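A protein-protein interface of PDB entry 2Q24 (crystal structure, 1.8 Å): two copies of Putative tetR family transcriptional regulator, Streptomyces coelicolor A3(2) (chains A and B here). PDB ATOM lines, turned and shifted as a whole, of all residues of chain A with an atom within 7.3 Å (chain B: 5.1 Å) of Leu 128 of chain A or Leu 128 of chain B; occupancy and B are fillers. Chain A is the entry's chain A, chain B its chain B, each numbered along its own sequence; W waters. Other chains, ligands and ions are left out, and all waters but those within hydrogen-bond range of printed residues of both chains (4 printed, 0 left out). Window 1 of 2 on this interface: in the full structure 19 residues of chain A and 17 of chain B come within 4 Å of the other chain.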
ATOM      1  N   ARG A  67       6.234   6.221 -12.504  1.00  0.00           N
ATOM      2  CA  ARG A  67       6.915   6.639 -13.735  1.00  0.00           C
ATOM      3  C   ARG A  67       8.342   6.103 -13.795  1.00  0.00           C
ATOM      4  O   ARG A  67       8.843   5.728 -14.857  1.00  0.00           O
ATOM      5  CB  ARG A  67       6.928   8.178 -13.799  1.00  0.00           C
ATOM      6  CG  ARG A  67       5.504   8.669 -14.144  1.00  0.00           C
ATOM      7  CD  ARG A  67       5.372  10.219 -14.118  1.00  0.00           C
ATOM      8  NE  ARG A  67       6.101  10.911 -15.203  1.00  0.00           N
ATOM      9  CZ  ARG A  67       6.097  12.232 -15.392  1.00  0.00           C
ATOM     10  NH1 ARG A  67       5.472  13.045 -14.533  1.00  0.00           N
ATOM     11  NH2 ARG A  67       6.773  12.759 -16.414  1.00  0.00           N
ATOM     12  N   VAL A  70       8.380   2.470 -14.830  1.00  0.00           N
ATOM     13  CA  VAL A  70       8.121   2.427 -16.284  1.00  0.00           C
ATOM     14  C   VAL A  70       9.406   2.770 -17.018  1.00  0.00           C
ATOM     15  O   VAL A  70       9.825   2.036 -17.922  1.00  0.00           O
ATOM     16  CB  VAL A  70       6.973   3.390 -16.713  1.00  0.00           C
ATOM     17  CG1 VAL A  70       6.865   3.500 -18.250  1.00  0.00           C
ATOM     18  CG2 VAL A  70       5.619   2.870 -16.172  1.00  0.00           C
ATOM     19  N   ALA A  71      10.071   3.854 -16.609  1.00  0.00           N
ATOM     20  CA  ALA A  71      11.277   4.260 -17.313  1.00  0.00           C
ATOM     21  C   ALA A  71      12.424   3.276 -17.158  1.00  0.00           C
ATOM     22  O   ALA A  71      13.114   2.992 -18.142  1.00  0.00           O
ATOM     23  CB  ALA A  71      11.721   5.693 -16.885  1.00  0.00           C
ATOM     24  N   ARG A  72      12.589   2.711 -15.970  1.00  0.00           N
ATOM     25  CA  ARG A  72      13.625   1.696 -15.781  1.00  0.00           C
ATOM     26  C   ARG A  72      13.389   0.462 -16.634  1.00  0.00           C
ATOM     27  O   ARG A  72      14.343  -0.088 -17.197  1.00  0.00           O
ATOM     28  CB  ARG A  72      13.824   1.350 -14.292  1.00  0.00           C
ATOM     29  CG  ARG A  72      14.540   2.501 -13.538  1.00  0.00           C
ATOM     30  CD  ARG A  72      14.640   2.128 -11.986  1.00  0.00           C
ATOM     31  NE  ARG A  72      14.317   0.714 -11.783  1.00  0.00           N
ATOM     32  CZ  ARG A  72      13.286   0.240 -11.087  1.00  0.00           C
ATOM     33  NH1 ARG A  72      12.449   1.040 -10.421  1.00  0.00           N
ATOM     34  NH2 ARG A  72      13.103  -1.060 -11.043  1.00  0.00           N
ATOM     35  N   CYS A  74      11.623   0.395 -19.590  1.00  0.00           N
ATOM     36  CA  CYS A  74      11.836   0.743 -21.002  1.00  0.00           C
ATOM     37  C   CYS A  74      13.296   0.964 -21.363  1.00  0.00           C
ATOM     38  O   CYS A  74      13.798   0.506 -22.417  1.00  0.00           O
ATOM     39  CB  CYS A  74      11.005   1.994 -21.440  1.00  0.00           C
ATOM     40  SG  CYS A  74       9.245   1.714 -21.244  1.00  0.00           S
ATOM     41  N   ASP A  75      14.015   1.606 -20.456  1.00  0.00           N
ATOM     42  CA  ASP A  75      15.386   2.012 -20.702  1.00  0.00           C
ATOM     43  C   ASP A  75      16.362   0.870 -20.517  1.00  0.00           C
ATOM     44  O   ASP A  75      17.518   1.034 -20.819  1.00  0.00           O
ATOM     45  CB  ASP A  75      15.775   3.171 -19.763  1.00  0.00           C
ATOM     46  CG  ASP A  75      14.969   4.452 -20.051  1.00  0.00           C
ATOM     47  OD1 ASP A  75      14.292   4.497 -21.078  1.00  0.00           O
ATOM     48  OD2 ASP A  75      14.996   5.353 -19.191  1.00  0.00           O
ATOM     49  N   TRP A  93      13.749  -9.316 -20.660  1.00  0.00           N
ATOM     50  CA  TRP A  93      12.932  -8.108 -20.508  1.00  0.00           C
ATOM     51  C   TRP A  93      11.534  -8.493 -20.044  1.00  0.00           C
ATOM     52  O   TRP A  93      10.911  -7.787 -19.228  1.00  0.00           O
ATOM     53  CB  TRP A  93      12.898  -7.325 -21.854  1.00  0.00           C
ATOM     54  CG  TRP A  93      12.154  -5.994 -21.751  1.00  0.00           C
ATOM     55  CD1 TRP A  93      12.678  -4.773 -21.344  1.00  0.00           C
ATOM     56  CD2 TRP A  93      10.763  -5.798 -21.942  1.00  0.00           C
ATOM     57  NE1 TRP A  93      11.680  -3.820 -21.334  1.00  0.00           N
ATOM     58  CE2 TRP A  93      10.496  -4.414 -21.702  1.00  0.00           C
ATOM     59  CE3 TRP A  93       9.705  -6.635 -22.345  1.00  0.00           C
ATOM     60  CZ2 TRP A  93       9.200  -3.859 -21.829  1.00  0.00           C
ATOM     61  CZ3 TRP A  93       8.409  -6.084 -22.438  1.00  0.00           C
ATOM     62  CH2 TRP A  93       8.183  -4.706 -22.217  1.00  0.00           C
ATOM     63  N   TYR A 122      -0.358   7.421 -14.986  1.00  0.00           N
ATOM     64  CA  TYR A 122      -0.076   6.549 -16.126  1.00  0.00           C
ATOM     65  C   TYR A 122       0.424   7.277 -17.362  1.00  0.00           C
ATOM     66  O   TYR A 122       1.314   6.765 -18.061  1.00  0.00           O
ATOM     67  CB  TYR A 122      -1.335   5.710 -16.458  1.00  0.00           C
ATOM     68  CG  TYR A 122      -1.746   4.890 -15.238  1.00  0.00           C
ATOM     69  CD1 TYR A 122      -0.838   4.024 -14.648  1.00  0.00           C
ATOM     70  CD2 TYR A 122      -2.980   5.079 -14.614  1.00  0.00           C
ATOM     71  CE1 TYR A 122      -1.159   3.296 -13.505  1.00  0.00           C
ATOM     72  CE2 TYR A 122      -3.321   4.337 -13.486  1.00  0.00           C
ATOM     73  CZ  TYR A 122      -2.396   3.447 -12.944  1.00  0.00           C
ATOM     74  OH  TYR A 122      -2.686   2.698 -11.825  1.00  0.00           O
ATOM     75  N   GLY A 123      -0.162   8.430 -17.659  1.00  0.00           N
ATOM     76  CA  GLY A 123       0.247   9.227 -18.852  1.00  0.00           C
ATOM     77  C   GLY A 123       0.386   8.327 -20.076  1.00  0.00           C
ATOM     78  O   GLY A 123      -0.538   7.599 -20.416  1.00  0.00           O
ATOM     79  N   ASP A 124       1.561   8.370 -20.715  1.00  0.00           N
ATOM     80  CA  ASP A 124       1.801   7.619 -21.945  1.00  0.00           C
ATOM     81  C   ASP A 124       2.602   6.354 -21.673  1.00  0.00           C
ATOM     82  O   ASP A 124       3.288   5.825 -22.573  1.00  0.00           O
ATOM     83  CB  ASP A 124       2.462   8.509 -23.037  1.00  0.00           C
ATOM     84  CG  ASP A 124       1.454   9.455 -23.734  1.00  0.00           C
ATOM     85  OD1 ASP A 124       1.184   9.288 -24.943  1.00  0.00           O
ATOM     86  OD2 ASP A 124       0.890  10.314 -23.095  1.00  0.00           O
ATOM     87  N   SER A 125       2.458   5.804 -20.463  1.00  0.00           N
ATOM     88  CA  SER A 125       3.261   4.628 -20.061  1.00  0.00           C
ATOM     89  C   SER A 125       3.006   3.440 -20.992  1.00  0.00           C
ATOM     90  O   SER A 125       3.963   2.733 -21.368  1.00  0.00           O
ATOM     91  CB  SER A 125       2.932   4.205 -18.619  1.00  0.00           C
ATOM     92  OG  SER A 125       3.350   5.219 -17.732  1.00  0.00           O
ATOM     93  N   ARG A 126       1.740   3.228 -21.368  1.00  0.00           N
ATOM     94  CA  ARG A 126       1.425   2.077 -22.221  1.00  0.00           C
ATOM     95  C   ARG A 126       2.172   2.220 -23.548  1.00  0.00           C
ATOM     96  O   ARG A 126       2.735   1.252 -24.038  1.00  0.00           O
ATOM     97  CB  ARG A 126      -0.086   1.946 -22.461  1.00  0.00           C
ATOM     98  CG  ARG A 126      -0.455   0.732 -23.317  1.00  0.00           C
ATOM     99  CD  ARG A 126      -1.970   0.798 -23.720  1.00  0.00           C
ATOM    100  N   GLN A 127       2.159   3.412 -24.137  1.00  0.00           N
ATOM    101  CA  GLN A 127       2.892   3.588 -25.410  1.00  0.00           C
ATOM    102  C   GLN A 127       4.413   3.398 -25.268  1.00  0.00           C
ATOM    103  O   GLN A 127       5.049   2.830 -26.164  1.00  0.00           O
ATOM    104  CB  GLN A 127       2.538   4.924 -26.001  1.00  0.00           C
ATOM    105  CG  GLN A 127       0.988   5.028 -26.325  1.00  0.00           C
ATOM    106  CD  GLN A 127       0.151   5.783 -25.274  1.00  0.00           C
ATOM    107  OE1 GLN A 127       0.248   5.544 -24.069  1.00  0.00           O
ATOM    108  NE2 GLN A 127      -0.698   6.700 -25.748  1.00  0.00           N
ATOM    109  N   LEU A 128       4.982   3.866 -24.160  1.00  0.00           N
ATOM    110  CA  LEU A 128       6.411   3.760 -23.932  1.00  0.00           C
ATOM    111  C   LEU A 128       6.819   2.289 -23.843  1.00  0.00           C
ATOM    112  O   LEU A 128       7.811   1.882 -24.419  1.00  0.00           O
ATOM    113  CB  LEU A 128       6.828   4.475 -22.602  1.00  0.00           C
ATOM    114  CG  LEU A 128       6.786   6.020 -22.655  1.00  0.00           C
ATOM    115  CD1 LEU A 128       6.876   6.595 -21.210  1.00  0.00           C
ATOM    116  CD2 LEU A 128       7.917   6.540 -23.556  1.00  0.00           C
ATOM    117  N   ILE A 129       6.039   1.532 -23.077  1.00  0.00           N
ATOM    118  CA  ILE A 129       6.328   0.095 -22.858  1.00  0.00           C
ATOM    119  C   ILE A 129       6.138  -0.691 -24.173  1.00  0.00           C
ATOM    120  O   ILE A 129       6.971  -1.540 -24.510  1.00  0.00           O
ATOM    121  CB  ILE A 129       5.429  -0.457 -21.777  1.00  0.00           C
ATOM    122  CG1 ILE A 129       5.829   0.190 -20.433  1.00  0.00           C
ATOM    123  CG2 ILE A 129       5.656  -1.998 -21.618  1.00  0.00           C
ATOM    124  CD1 ILE A 129       4.854  -0.236 -19.213  1.00  0.00           C
ATOM    125  N   GLN A 130       5.080  -0.382 -24.887  1.00  0.00           N
ATOM    126  CA  GLN A 130       4.869  -0.972 -26.215  1.00  0.00           C
ATOM    127  C   GLN A 130       6.018  -0.711 -27.169  1.00  0.00           C
ATOM    128  O   GLN A 130       6.438  -1.601 -27.921  1.00  0.00           O
ATOM    129  CB  GLN A 130       3.571  -0.465 -26.831  1.00  0.00           C
ATOM    130  CG  GLN A 130       3.311  -1.026 -28.202  1.00  0.00           C
ATOM    131  CD  GLN A 130       3.071  -2.511 -28.202  1.00  0.00           C
ATOM    132  OE1 GLN A 130       3.995  -3.259 -28.556  1.00  0.00           O
ATOM    133  N   SER A 131       6.566   0.495 -27.138  1.00  0.00           N
ATOM    134  CA  SER A 131       7.681   0.787 -28.004  1.00  0.00           C
ATOM    135  C   SER A 131       8.943  -0.013 -27.599  1.00  0.00           C
ATOM    136  O   SER A 131       9.734  -0.445 -28.470  1.00  0.00           O
ATOM    137  CB  SER A 131       7.934   2.290 -28.014  1.00  0.00           C
ATOM    138  OG  SER A 131       8.857   2.633 -29.046  1.00  0.00           O
ATOM    139  N   ALA A 132       9.119  -0.253 -26.293  1.00  0.00           N
ATOM    140  CA  ALA A 132      10.309  -0.979 -25.825  1.00  0.00           C
ATOM    141  C   ALA A 132      10.156  -2.391 -26.332  1.00  0.00           C
ATOM    142  O   ALA A 132      11.089  -2.997 -26.841  1.00  0.00           O
ATOM    143  CB  ALA A 132      10.384  -0.956 -24.260  1.00  0.00           C
ATOM    144  N   LEU A 133       8.950  -2.913 -26.235  1.00  0.00           N
ATOM    145  CA  LEU A 133       8.712  -4.283 -26.748  1.00  0.00           C
ATOM    146  C   LEU A 133       8.940  -4.370 -28.259  1.00  0.00           C
ATOM    147  O   LEU A 133       9.539  -5.337 -28.776  1.00  0.00           O
ATOM    148  CB  LEU A 133       7.267  -4.685 -26.366  1.00  0.00           C
ATOM    149  CG  LEU A 133       6.819  -6.070 -26.768  1.00  0.00           C
ATOM    150  CD1 LEU A 133       7.772  -7.104 -26.159  1.00  0.00           C
ATOM    151  CD2 LEU A 133       5.385  -6.317 -26.254  1.00  0.00           C
ATOM    152  N   THR A 134       8.465  -3.364 -28.987  1.00  0.00           N
ATOM    153  CA  THR A 134       8.694  -3.314 -30.417  1.00  0.00           C
ATOM    154  C   THR A 134      10.169  -3.317 -30.758  1.00  0.00           C
ATOM    155  O   THR A 134      10.577  -4.024 -31.692  1.00  0.00           O
ATOM    156  CB  THR A 134       8.000  -2.050 -31.039  1.00  0.00           C
ATOM    157  OG1 THR A 134       6.599  -2.115 -30.744  1.00  0.00           O
ATOM    158  CG2 THR A 134       8.224  -2.006 -32.607  1.00  0.00           C
ATOM    159  N   PHE A 156       2.072  -7.300 -26.455  1.00  0.00           N
ATOM    160  CA  PHE A 156       1.814  -6.473 -25.284  1.00  0.00           C
ATOM    161  C   PHE A 156       0.548  -6.955 -24.572  1.00  0.00           C
ATOM    162  O   PHE A 156       0.543  -7.072 -23.344  1.00  0.00           O
ATOM    163  CB  PHE A 156       1.759  -4.963 -25.609  1.00  0.00           C
ATOM    164  CG  PHE A 156       1.526  -4.105 -24.400  1.00  0.00           C
ATOM    165  CD1 PHE A 156       2.588  -3.636 -23.648  1.00  0.00           C
ATOM    166  CD2 PHE A 156       0.213  -3.804 -23.967  1.00  0.00           C
ATOM    167  CE1 PHE A 156       2.372  -2.855 -22.479  1.00  0.00           C
ATOM    168  CE2 PHE A 156      -0.004  -3.038 -22.795  1.00  0.00           C
ATOM    169  CZ  PHE A 156       1.093  -2.571 -22.050  1.00  0.00           C
ATOM    170  N   VAL B  70       7.210  14.032 -24.998  1.00  0.00           N
ATOM    171  CA  VAL B  70       8.378  13.177 -24.670  1.00  0.00           C
ATOM    172  C   VAL B  70       8.161  11.764 -25.203  1.00  0.00           C
ATOM    173  O   VAL B  70       9.039  11.198 -25.845  1.00  0.00           O
ATOM    174  CB  VAL B  70       8.590  13.149 -23.134  1.00  0.00           C
ATOM    175  CG1 VAL B  70       9.664  12.075 -22.716  1.00  0.00           C
ATOM    176  CG2 VAL B  70       9.036  14.580 -22.659  1.00  0.00           C
ATOM    177  N   ALA B  71       7.004  11.168 -24.930  1.00  0.00           N
ATOM    178  CA  ALA B  71       6.790   9.787 -25.338  1.00  0.00           C
ATOM    179  C   ALA B  71       6.771   9.666 -26.863  1.00  0.00           C
ATOM    180  O   ALA B  71       7.364   8.732 -27.428  1.00  0.00           O
ATOM    181  CB  ALA B  71       5.516   9.245 -24.735  1.00  0.00           C
ATOM    182  N   CYS B  74      10.437   9.651 -27.990  1.00  0.00           N
ATOM    183  CA  CYS B  74      11.107   8.410 -27.686  1.00  0.00           C
ATOM    184  C   CYS B  74      10.642   7.231 -28.536  1.00  0.00           C
ATOM    185  O   CYS B  74      11.442   6.417 -28.997  1.00  0.00           O
ATOM    186  CB  CYS B  74      10.980   8.082 -26.177  1.00  0.00           C
ATOM    187  SG  CYS B  74      11.833   9.293 -25.140  1.00  0.00           S
ATOM    188  N   ASP B  75       9.355   7.213 -28.808  1.00  0.00           N
ATOM    189  CA  ASP B  75       8.722   6.049 -29.390  1.00  0.00           C
ATOM    190  C   ASP B  75       8.880   6.071 -30.926  1.00  0.00           C
ATOM    191  O   ASP B  75       8.459   5.141 -31.572  1.00  0.00           O
ATOM    192  CB  ASP B  75       7.243   6.070 -28.998  1.00  0.00           C
ATOM    193  CG  ASP B  75       7.006   5.710 -27.497  1.00  0.00           C
ATOM    194  OD1 ASP B  75       7.919   5.268 -26.829  1.00  0.00           O
ATOM    195  OD2 ASP B  75       5.884   5.930 -27.024  1.00  0.00           O
ATOM    196  N   ASP B 124      10.841  10.987 -15.365  1.00  0.00           N
ATOM    197  CA  ASP B 124      12.071  10.355 -15.881  1.00  0.00           C
ATOM    198  C   ASP B 124      12.305  10.753 -17.330  1.00  0.00           C
ATOM    199  O   ASP B 124      12.939  10.002 -18.073  1.00  0.00           O
ATOM    200  CB  ASP B 124      11.979   8.816 -15.720  1.00  0.00           C
ATOM    201  CG  ASP B 124      12.431   8.347 -14.274  1.00  0.00           C
ATOM    202  OD1 ASP B 124      13.470   7.676 -14.125  1.00  0.00           O
ATOM    203  OD2 ASP B 124      11.797   8.707 -13.304  1.00  0.00           O
ATOM    204  N   SER B 125      11.725  11.884 -17.773  1.00  0.00           N
ATOM    205  CA  SER B 125      11.894  12.291 -19.221  1.00  0.00           C
ATOM    206  C   SER B 125      13.354  12.315 -19.719  1.00  0.00           C
ATOM    207  O   SER B 125      13.635  11.844 -20.827  1.00  0.00           O
ATOM    208  CB  SER B 125      11.228  13.654 -19.558  1.00  0.00           C
ATOM    209  OG  SER B 125       9.888  13.615 -19.158  1.00  0.00           O
ATOM    210  N   ARG B 126      14.253  12.876 -18.920  1.00  0.00           N
ATOM    211  CA  ARG B 126      15.641  12.961 -19.322  1.00  0.00           C
ATOM    212  C   ARG B 126      16.180  11.540 -19.586  1.00  0.00           C
ATOM    213  O   ARG B 126      16.869  11.312 -20.573  1.00  0.00           O
ATOM    214  CB  ARG B 126      16.493  13.718 -18.284  1.00  0.00           C
ATOM    215  CG  ARG B 126      17.967  13.874 -18.706  1.00  0.00           C
ATOM    216  CD  ARG B 126      18.795  14.408 -17.546  1.00  0.00           C
ATOM    217  N   GLN B 127      15.896  10.611 -18.690  1.00  0.00           N
ATOM    218  CA  GLN B 127      16.379   9.227 -18.818  1.00  0.00           C
ATOM    219  C   GLN B 127      15.781   8.547 -20.058  1.00  0.00           C
ATOM    220  O   GLN B 127      16.466   7.822 -20.785  1.00  0.00           O
ATOM    221  CB  GLN B 127      16.019   8.429 -17.553  1.00  0.00           C
ATOM    222  CG  GLN B 127      16.591   9.022 -16.247  1.00  0.00           C
ATOM    223  CD  GLN B 127      15.645   9.972 -15.483  1.00  0.00           C
ATOM    224  OE1 GLN B 127      15.249  11.045 -15.967  1.00  0.00           O
ATOM    225  NE2 GLN B 127      15.325   9.585 -14.248  1.00  0.00           N
ATOM    226  N   LEU B 128      14.480   8.723 -20.260  1.00  0.00           N
ATOM    227  CA  LEU B 128      13.794   8.101 -21.415  1.00  0.00           C
ATOM    228  C   LEU B 128      14.433   8.607 -22.727  1.00  0.00           C
ATOM    229  O   LEU B 128      14.729   7.828 -23.653  1.00  0.00           O
ATOM    230  CB  LEU B 128      12.301   8.465 -21.392  1.00  0.00           C
ATOM    231  CG  LEU B 128      11.429   7.833 -20.290  1.00  0.00           C
ATOM    232  CD1 LEU B 128      10.064   8.556 -20.251  1.00  0.00           C
ATOM    233  CD2 LEU B 128      11.238   6.367 -20.602  1.00  0.00           C
ATOM    234  N   ILE B 129      14.640   9.927 -22.794  1.00  0.00           N
ATOM    235  CA  ILE B 129      15.153  10.519 -24.039  1.00  0.00           C
ATOM    236  C   ILE B 129      16.617  10.163 -24.222  1.00  0.00           C
ATOM    237  O   ILE B 129      17.050   9.843 -25.317  1.00  0.00           O
ATOM    238  CB  ILE B 129      15.042  12.029 -24.004  1.00  0.00           C
ATOM    239  CG1 ILE B 129      13.555  12.422 -24.064  1.00  0.00           C
ATOM    240  CG2 ILE B 129      15.833  12.620 -25.208  1.00  0.00           C
ATOM    241  CD1 ILE B 129      13.300  13.878 -23.666  1.00  0.00           C
ATOM    242  N   GLN B 130      17.376  10.195 -23.155  1.00  0.00           N
ATOM    243  CA  GLN B 130      18.783   9.683 -23.261  1.00  0.00           C
ATOM    244  C   GLN B 130      18.862   8.229 -23.747  1.00  0.00           C
ATOM    245  O   GLN B 130      19.764   7.847 -24.534  1.00  0.00           O
ATOM    246  CB  GLN B 130      19.542   9.905 -21.972  1.00  0.00           C
ATOM    247  CG  GLN B 130      20.001  11.371 -21.910  1.00  0.00           C
ATOM    248  CD  GLN B 130      20.753  11.769 -20.624  1.00  0.00           C
ATOM    249  OE1 GLN B 130      21.056  12.959 -20.376  1.00  0.00           O
ATOM    250  NE2 GLN B 130      21.048  10.789 -19.817  1.00  0.00           N
ATOM    251  N   SER B 131      17.905   7.399 -23.323  1.00  0.00           N
ATOM    252  CA  SER B 131      17.913   6.009 -23.755  1.00  0.00           C
ATOM    253  C   SER B 131      17.563   5.868 -25.214  1.00  0.00           C
ATOM    254  O   SER B 131      18.109   5.013 -25.892  1.00  0.00           O
ATOM    255  CB  SER B 131      16.973   5.177 -22.874  1.00  0.00           C
ATOM    256  OG  SER B 131      17.132   3.785 -23.133  1.00  0.00           O
ATOM    257  N   ALA B 132      16.671   6.737 -25.707  1.00  0.00           N
ATOM    258  CA  ALA B 132      16.291   6.738 -27.142  1.00  0.00           C
ATOM    259  C   ALA B 132      17.530   7.090 -27.961  1.00  0.00           C
ATOM    260  O   ALA B 132      17.822   6.496 -28.997  1.00  0.00           O
ATOM    261  CB  ALA B 132      15.190   7.782 -27.373  1.00  0.00           C
HETATM  262  O   HOH W   1       8.454   9.896 -16.832  1.00  0.00           O
HETATM  263  O   HOH W   2       7.975  11.609 -19.019  1.00  0.00           O
HETATM  264  O   HOH W   3      19.599   3.319 -22.036  1.00  0.00           O
HETATM  265  O   HOH W   4       7.312   2.121 -31.365  1.00  0.00           O
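Printed residues of chain B that touch a printed residue of chain A: Ala 71, Asp 75, Asp 124, Gln 127, Leu 128 and Ser 131.
Hydrophobic or aromatic side chains of chain B that line the printed part of chain A: Ala 71 and Leu 128.
Of the 21 printed residues of chain A, 6 touch a printed residue of chain B.
Hydrophobic or aromatic side chains of chain A that line the printed part of chain B: Ala 71 and Leu 128.
Among the printed residues, no Asp or Glu carboxylate lies within 4 Å of a Lys or Arg side-chain nitrogen of the other chain.
The side-chain sulfur (SG) of Cys 74 of chain A is in hydrogen-bond range of the backbone carbonyl oxygen (O) of Leu 128 of chain A.
OD1 of Asp 124 of chain A sits at hydrogen-bond distance from NE2 of Gln 127 of chain A, 3.3 Å away.
The side-chain sulfur (SG) of Cys 74 of chain B lies within hydrogen-bond range of the backbone carbonyl oxygen (O) of Leu 128 of chain B.
The side-chain amide nitrogen (NE2) of Gln 127 of chain B lies within hydrogen-bond range of the side-chain carboxylate (OD1) of Asp 124 of chain B (2.7 Å).
Ala 71 of chain A touches Leu 128 of chain B, and with the chains exchanged Leu 128 of chain A touches Ala 71 of chain B.
Asp 75 of chain A touches Gln 127 of chain B, and with the chains exchanged Gln 127 of chain A touches Asp 75 of chain B.
Asp 75 of chain A touches Ser 131 of chain B, and with the chains exchanged Ser 131 of chain A touches Asp 75 of chain B.
Leu 128 of chain A touches its own counterpart, Leu 128 of chain B.
13 positions are printed for both chains.
Of the 11 pairs that touch across the chains among the printed residues, 11 have their exchanged pair printed and touching as well.
Asp 124 of chain B touches Ala 71 of chain A.
Leu 128 of chain B touches Ala 71 of chain A.
Asp 75 of chain A touches Leu 128 of chain B.
Asp 75 of chain A touches Ser 131 of chain B (OD1 to CB, 3.3 Å).
Asp 124 of chain A touches Ala 71 of chain B.
Ala 71 of chain B touches Leu 128 of chain A (CB to CD2, 3.8 Å).
Asp 75 of chain B touches Leu 128 of chain A.
CD1 of Leu 128 of chain B touches CD1 of Leu 128 of chain A, at 3.9 Å.
Asp 75 of chain B touches Ser 131 of chain A.
Of chain B, only Ala 71 (3.8 Å), Asp 75 (3.5 Å) and Leu 128 (3.9 Å) come within 4 Å of Leu 128 of chain A.
Leu 128 of chain B touches three residues of chain A.
Of the printed residues of chain A, Asp 75 of chain B touches Gln 127, Leu 128 and Ser 131.
Of the printed residues of chain A, Ser 131 of chain B touches Asp 75.
Of the printed residues of chain B, Ala 71 of chain A touches Asp 124 and Leu 128.
The nearest printed residue of chain B that does not touch Ser 131 of chain A is Cys 74 of chain B (4.6 Å).
The backbone carbonyl oxygen (O) of Gln 127 of chain B sits close to the side-chain carboxylate (OD2) of Asp 75 of chain A (3.3 Å).
O of Gln 127 of chain A sits close to OD2 of Asp 75 of chain B, 3.3 Å away.
Water W3 lies within hydrogen-bond range of OG of Ser 131 of chain B (2.7 Å) and O of Asp 75 of chain A (3.3 Å).
Water W2 bridges the side-chain hydroxyl of Ser 125 of chain B (2.8 Å) and the guanidinium group of Arg 67 of chain A (3.1 Å).
Water W4 lies within hydrogen-bond range of OG of Ser 131 of chain A (2.8 Å) and O of Asp 75 of chain B (3.2 Å).
Water W1 bridges N of Asp 124 of chain B (3.0 Å) and NE of Arg 67 of chain A (3.0 Å).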
